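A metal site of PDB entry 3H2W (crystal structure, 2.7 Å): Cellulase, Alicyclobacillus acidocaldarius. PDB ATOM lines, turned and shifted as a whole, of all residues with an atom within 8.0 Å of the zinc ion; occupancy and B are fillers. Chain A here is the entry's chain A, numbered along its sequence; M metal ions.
O of Cys 104 sits close to N of Gly 139 (3.4 Å). The side-chain carboxylate (OD2) of Asp 231 is in hydrogen-bond range of a ring nitrogen (NE2) of His 122 (2.8 Å). The backbone carbonyl oxygen (O) of Gly 140 lies within hydrogen-bond range of the backbone NH (N) of Cys 104, at 2.8 Å. The backbone carbonyl oxygen (O) of Cys 121 lies close to the backbone NH (N) of Gly 105 (3.2 Å). The backbone NH of His 142 is in hydrogen-bond range of the backbone carbonyl oxygen of Gln 102 (2.7 Å).
The zinc ion is bound by ND1 of His 122, NE2 of His 142, SG of Cys 104 and SG of Cys 121.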
ATOM      1  N   GLN A 102      14.040   5.817  31.733  1.00  0.00           N
ATOM      2  CA  GLN A 102      14.786   6.456  30.640  1.00  0.00           C
ATOM      3  C   GLN A 102      16.241   5.969  30.508  1.00  0.00           C
ATOM      4  O   GLN A 102      16.958   6.457  29.637  1.00  0.00           O
ATOM      5  CB  GLN A 102      14.820   7.979  30.838  1.00  0.00           C
ATOM      6  CG  GLN A 102      13.476   8.669  30.693  1.00  0.00           C
ATOM      7  CD  GLN A 102      12.905   8.522  29.304  1.00  0.00           C
ATOM      8  OE1 GLN A 102      12.261   7.535  29.002  1.00  0.00           O
ATOM      9  NE2 GLN A 102      13.157   9.502  28.441  1.00  0.00           N
ATOM     10  N   LEU A 103      16.684   5.022  31.340  1.00  0.00           N
ATOM     11  CA  LEU A 103      18.101   4.623  31.316  1.00  0.00           C
ATOM     12  C   LEU A 103      18.512   4.000  29.986  1.00  0.00           C
ATOM     13  O   LEU A 103      17.822   3.148  29.415  1.00  0.00           O
ATOM     14  CB  LEU A 103      18.454   3.672  32.471  1.00  0.00           C
ATOM     15  CG  LEU A 103      18.694   4.260  33.876  1.00  0.00           C
ATOM     16  CD1 LEU A 103      18.742   3.108  34.808  1.00  0.00           C
ATOM     17  CD2 LEU A 103      19.943   5.100  33.995  1.00  0.00           C
ATOM     18  N   CYS A 104      19.670   4.442  29.510  1.00  0.00           N
ATOM     19  CA  CYS A 104      20.289   3.973  28.289  1.00  0.00           C
ATOM     20  C   CYS A 104      21.435   2.976  28.572  1.00  0.00           C
ATOM     21  O   CYS A 104      22.281   3.200  29.435  1.00  0.00           O
ATOM     22  CB  CYS A 104      20.858   5.171  27.512  1.00  0.00           C
ATOM     23  SG  CYS A 104      21.234   4.772  25.819  1.00  0.00           S
ATOM     24  N   GLY A 105      21.436   1.876  27.845  1.00  0.00           N
ATOM     25  CA  GLY A 105      22.509   0.875  27.934  1.00  0.00           C
ATOM     26  C   GLY A 105      22.546   0.063  29.214  1.00  0.00           C
ATOM     27  O   GLY A 105      23.605  -0.336  29.667  1.00  0.00           O
ATOM     28  N   VAL A 106      21.384  -0.198  29.788  1.00  0.00           N
ATOM     29  CA  VAL A 106      21.337  -1.061  30.936  1.00  0.00           C
ATOM     30  C   VAL A 106      20.038  -1.906  30.927  1.00  0.00           C
ATOM     31  O   VAL A 106      18.933  -1.386  30.749  1.00  0.00           O
ATOM     32  CB  VAL A 106      21.518  -0.279  32.264  1.00  0.00           C
ATOM     33  CG1 VAL A 106      22.995   0.150  32.463  1.00  0.00           C
ATOM     34  CG2 VAL A 106      20.631   0.920  32.261  1.00  0.00           C
ATOM     35  N   HIS A 118      13.071  -3.750  29.605  1.00  0.00           N
ATOM     36  CA  HIS A 118      13.757  -4.013  28.361  1.00  0.00           C
ATOM     37  C   HIS A 118      15.256  -4.172  28.524  1.00  0.00           C
ATOM     38  O   HIS A 118      15.828  -3.927  29.609  1.00  0.00           O
ATOM     39  CB  HIS A 118      13.469  -2.909  27.341  1.00  0.00           C
ATOM     40  CG  HIS A 118      14.136  -1.600  27.647  1.00  0.00           C
ATOM     41  ND1 HIS A 118      15.494  -1.394  27.493  1.00  0.00           N
ATOM     42  CD2 HIS A 118      13.616  -0.412  28.032  1.00  0.00           C
ATOM     43  CE1 HIS A 118      15.792  -0.144  27.813  1.00  0.00           C
ATOM     44  NE2 HIS A 118      14.671   0.475  28.137  1.00  0.00           N
ATOM     45  N   GLY A 119      15.899  -4.576  27.425  1.00  0.00           N
ATOM     46  CA  GLY A 119      17.326  -4.850  27.401  1.00  0.00           C
ATOM     47  C   GLY A 119      18.124  -3.624  27.038  1.00  0.00           C
ATOM     48  O   GLY A 119      17.551  -2.600  26.649  1.00  0.00           O
ATOM     49  N   ALA A 120      19.454  -3.751  27.163  1.00  0.00           N
ATOM     50  CA  ALA A 120      20.374  -2.618  26.972  1.00  0.00           C
ATOM     51  C   ALA A 120      20.222  -2.091  25.575  1.00  0.00           C
ATOM     52  O   ALA A 120      20.083  -2.860  24.643  1.00  0.00           O
ATOM     53  CB  ALA A 120      21.819  -3.040  27.207  1.00  0.00           C
ATOM     54  N   CYS A 121      20.195  -0.773  25.434  1.00  0.00           N
ATOM     55  CA  CYS A 121      20.117  -0.156  24.126  1.00  0.00           C
ATOM     56  C   CYS A 121      21.354   0.711  23.915  1.00  0.00           C
ATOM     57  O   CYS A 121      22.098   0.990  24.856  1.00  0.00           O
ATOM     58  CB  CYS A 121      18.847   0.691  24.012  1.00  0.00           C
ATOM     59  SG  CYS A 121      18.620   1.892  25.331  1.00  0.00           S
ATOM     60  N   HIS A 122      21.593   1.092  22.663  1.00  0.00           N
ATOM     61  CA  HIS A 122      22.647   2.032  22.298  1.00  0.00           C
ATOM     62  C   HIS A 122      24.007   1.714  22.911  1.00  0.00           C
ATOM     63  O   HIS A 122      24.744   2.633  23.252  1.00  0.00           O
ATOM     64  CB  HIS A 122      22.211   3.455  22.654  1.00  0.00           C
ATOM     65  CG  HIS A 122      20.825   3.776  22.213  1.00  0.00           C
ATOM     66  ND1 HIS A 122      19.744   3.791  23.070  1.00  0.00           N
ATOM     67  CD2 HIS A 122      20.324   4.057  20.983  1.00  0.00           C
ATOM     68  CE1 HIS A 122      18.647   4.067  22.394  1.00  0.00           C
ATOM     69  NE2 HIS A 122      18.966   4.230  21.123  1.00  0.00           N
ATOM     70  N   THR A 123      24.348   0.424  23.009  1.00  0.00           N
ATOM     71  CA  THR A 123      25.618  -0.016  23.612  1.00  0.00           C
ATOM     72  C   THR A 123      26.869   0.153  22.708  1.00  0.00           C
ATOM     73  O   THR A 123      28.010  -0.113  23.137  1.00  0.00           O
ATOM     74  CB  THR A 123      25.555  -1.488  23.978  1.00  0.00           C
ATOM     75  OG1 THR A 123      25.330  -2.240  22.772  1.00  0.00           O
ATOM     76  CG2 THR A 123      24.453  -1.763  24.999  1.00  0.00           C
ATOM     77  N   GLY A 139      25.125   4.951  29.156  1.00  0.00           N
ATOM     78  CA  GLY A 139      24.446   5.257  30.401  1.00  0.00           C
ATOM     79  C   GLY A 139      23.750   6.585  30.294  1.00  0.00           C
ATOM     80  O   GLY A 139      23.729   7.197  29.232  1.00  0.00           O
ATOM     81  N   GLY A 140      23.193   7.028  31.404  1.00  0.00           N
ATOM     82  CA  GLY A 140      22.366   8.215  31.421  1.00  0.00           C
ATOM     83  C   GLY A 140      20.978   7.951  30.879  1.00  0.00           C
ATOM     84  O   GLY A 140      20.557   6.811  30.694  1.00  0.00           O
ATOM     85  N   TRP A 141      20.269   9.035  30.594  1.00  0.00           N
ATOM     86  CA  TRP A 141      18.852   9.009  30.259  1.00  0.00           C
ATOM     87  C   TRP A 141      18.584   9.311  28.780  1.00  0.00           C
ATOM     88  O   TRP A 141      19.237  10.162  28.163  1.00  0.00           O
ATOM     89  CB  TRP A 141      18.101  10.024  31.107  1.00  0.00           C
ATOM     90  CG  TRP A 141      18.316   9.863  32.585  1.00  0.00           C
ATOM     91  CD1 TRP A 141      18.358   8.692  33.282  1.00  0.00           C
ATOM     92  CD2 TRP A 141      18.500  10.902  33.547  1.00  0.00           C
ATOM     93  NE1 TRP A 141      18.553   8.937  34.613  1.00  0.00           N
ATOM     94  CE2 TRP A 141      18.644  10.285  34.801  1.00  0.00           C
ATOM     95  CE3 TRP A 141      18.550  12.295  33.480  1.00  0.00           C
ATOM     96  CZ2 TRP A 141      18.854  11.006  35.971  1.00  0.00           C
ATOM     97  CZ3 TRP A 141      18.742  13.012  34.639  1.00  0.00           C
ATOM     98  CH2 TRP A 141      18.891  12.359  35.871  1.00  0.00           C
ATOM     99  N   HIS A 142      17.606   8.632  28.226  1.00  0.00           N
ATOM    100  CA  HIS A 142      16.993   9.130  27.020  1.00  0.00           C
ATOM    101  C   HIS A 142      16.360  10.443  27.433  1.00  0.00           C
ATOM    102  O   HIS A 142      15.718  10.532  28.478  1.00  0.00           O
ATOM    103  CB  HIS A 142      15.978   8.152  26.475  1.00  0.00           C
ATOM    104  CG  HIS A 142      16.565   6.827  26.143  1.00  0.00           C
ATOM    105  ND1 HIS A 142      15.860   5.647  26.226  1.00  0.00           N
ATOM    106  CD2 HIS A 142      17.820   6.488  25.753  1.00  0.00           C
ATOM    107  CE1 HIS A 142      16.643   4.649  25.875  1.00  0.00           C
ATOM    108  NE2 HIS A 142      17.839   5.123  25.593  1.00  0.00           N
ATOM    109  N   ASP A 146      12.407  10.663  22.389  1.00  0.00           N
ATOM    110  CA  ASP A 146      13.434  10.130  21.502  1.00  0.00           C
ATOM    111  C   ASP A 146      14.504   9.488  22.371  1.00  0.00           C
ATOM    112  O   ASP A 146      14.372   9.445  23.582  1.00  0.00           O
ATOM    113  CB  ASP A 146      14.068  11.277  20.714  1.00  0.00           C
ATOM    114  CG  ASP A 146      14.960  12.156  21.581  1.00  0.00           C
ATOM    115  OD1 ASP A 146      14.629  12.334  22.774  1.00  0.00           O
ATOM    116  OD2 ASP A 146      16.006  12.627  21.085  1.00  0.00           O
ATOM    117  N   TYR A 147      15.570   9.035  21.739  1.00  0.00           N
ATOM    118  CA  TYR A 147      16.602   8.315  22.437  1.00  0.00           C
ATOM    119  C   TYR A 147      17.897   9.080  22.456  1.00  0.00           C
ATOM    120  O   TYR A 147      18.941   8.517  22.679  1.00  0.00           O
ATOM    121  CB  TYR A 147      16.817   6.944  21.813  1.00  0.00           C
ATOM    122  CG  TYR A 147      15.598   6.045  21.858  1.00  0.00           C
ATOM    123  CD1 TYR A 147      14.962   5.771  23.057  1.00  0.00           C
ATOM    124  CD2 TYR A 147      15.091   5.467  20.710  1.00  0.00           C
ATOM    125  CE1 TYR A 147      13.837   4.960  23.101  1.00  0.00           C
ATOM    126  CE2 TYR A 147      13.967   4.653  20.743  1.00  0.00           C
ATOM    127  CZ  TYR A 147      13.337   4.415  21.956  1.00  0.00           C
ATOM    128  OH  TYR A 147      12.222   3.595  22.002  1.00  0.00           O
ATOM    129  N   GLY A 148      17.838  10.387  22.241  1.00  0.00           N
ATOM    130  CA  GLY A 148      19.041  11.189  22.344  1.00  0.00           C
ATOM    131  C   GLY A 148      19.426  11.434  23.791  1.00  0.00           C
ATOM    132  O   GLY A 148      18.626  11.275  24.714  1.00  0.00           O
ATOM    133  N   LYS A 149      20.677  11.798  23.990  1.00  0.00           N
ATOM    134  CA  LYS A 149      21.159  12.275  25.275  1.00  0.00           C
ATOM    135  C   LYS A 149      21.877  13.610  25.030  1.00  0.00           C
ATOM    136  O   LYS A 149      22.870  13.672  24.289  1.00  0.00           O
ATOM    137  CB  LYS A 149      22.092  11.245  25.916  1.00  0.00           C
ATOM    138  CG  LYS A 149      21.480   9.844  25.961  1.00  0.00           C
ATOM    139  CD  LYS A 149      22.287   8.888  26.797  1.00  0.00           C
ATOM    140  CE  LYS A 149      23.512   8.351  26.048  1.00  0.00           C
ATOM    141  NZ  LYS A 149      24.135   7.192  26.779  1.00  0.00           N
ATOM    142  N   PRO A 228      13.687   0.807  22.093  1.00  0.00           N
ATOM    143  CA  PRO A 228      15.050   1.269  22.404  1.00  0.00           C
ATOM    144  C   PRO A 228      16.122   0.277  21.971  1.00  0.00           C
ATOM    145  O   PRO A 228      17.132   0.691  21.382  1.00  0.00           O
ATOM    146  CB  PRO A 228      15.045   1.380  23.943  1.00  0.00           C
ATOM    147  CG  PRO A 228      13.903   0.567  24.380  1.00  0.00           C
ATOM    148  CD  PRO A 228      12.861   0.734  23.312  1.00  0.00           C
ATOM    149  N   GLU A 229      15.893  -1.012  22.241  1.00  0.00           N
ATOM    150  CA  GLU A 229      16.868  -2.061  21.926  1.00  0.00           C
ATOM    151  C   GLU A 229      16.968  -2.369  20.406  1.00  0.00           C
ATOM    152  O   GLU A 229      18.010  -2.869  19.959  1.00  0.00           O
ATOM    153  CB  GLU A 229      16.583  -3.324  22.743  1.00  0.00           C
ATOM    154  CG  GLU A 229      15.238  -3.992  22.433  1.00  0.00           C
ATOM    155  CD  GLU A 229      14.261  -4.021  23.614  1.00  0.00           C
ATOM    156  OE1 GLU A 229      13.321  -3.198  23.648  1.00  0.00           O
ATOM    157  OE2 GLU A 229      14.432  -4.900  24.491  1.00  0.00           O
ATOM    158  N   ASP A 231      16.861   0.023  18.052  1.00  0.00           N
ATOM    159  CA  ASP A 231      17.383   1.245  17.418  1.00  0.00           C
ATOM    160  C   ASP A 231      18.849   1.067  17.001  1.00  0.00           C
ATOM    161  O   ASP A 231      19.773   1.270  17.805  1.00  0.00           O
ATOM    162  CB  ASP A 231      17.193   2.398  18.391  1.00  0.00           C
ATOM    163  CG  ASP A 231      17.658   3.723  17.849  1.00  0.00           C
ATOM    164  OD1 ASP A 231      17.914   3.846  16.633  1.00  0.00           O
ATOM    165  OD2 ASP A 231      17.753   4.658  18.672  1.00  0.00           O
ATOM    166  N   LEU A 235      25.676   6.194  16.258  1.00  0.00           N
ATOM    167  CA  LEU A 235      25.613   7.256  17.247  1.00  0.00           C
ATOM    168  C   LEU A 235      26.644   8.293  16.938  1.00  0.00           C
ATOM    169  O   LEU A 235      27.800   7.951  16.755  1.00  0.00           O
ATOM    170  CB  LEU A 235      25.931   6.687  18.644  1.00  0.00           C
ATOM    171  CG  LEU A 235      24.918   5.756  19.312  1.00  0.00           C
ATOM    172  CD1 LEU A 235      25.413   5.352  20.708  1.00  0.00           C
ATOM    173  CD2 LEU A 235      23.526   6.413  19.367  1.00  0.00           C
HETATM  174 ZN    ZN M   1      19.464   3.929  24.933  1.00  0.00          ZN
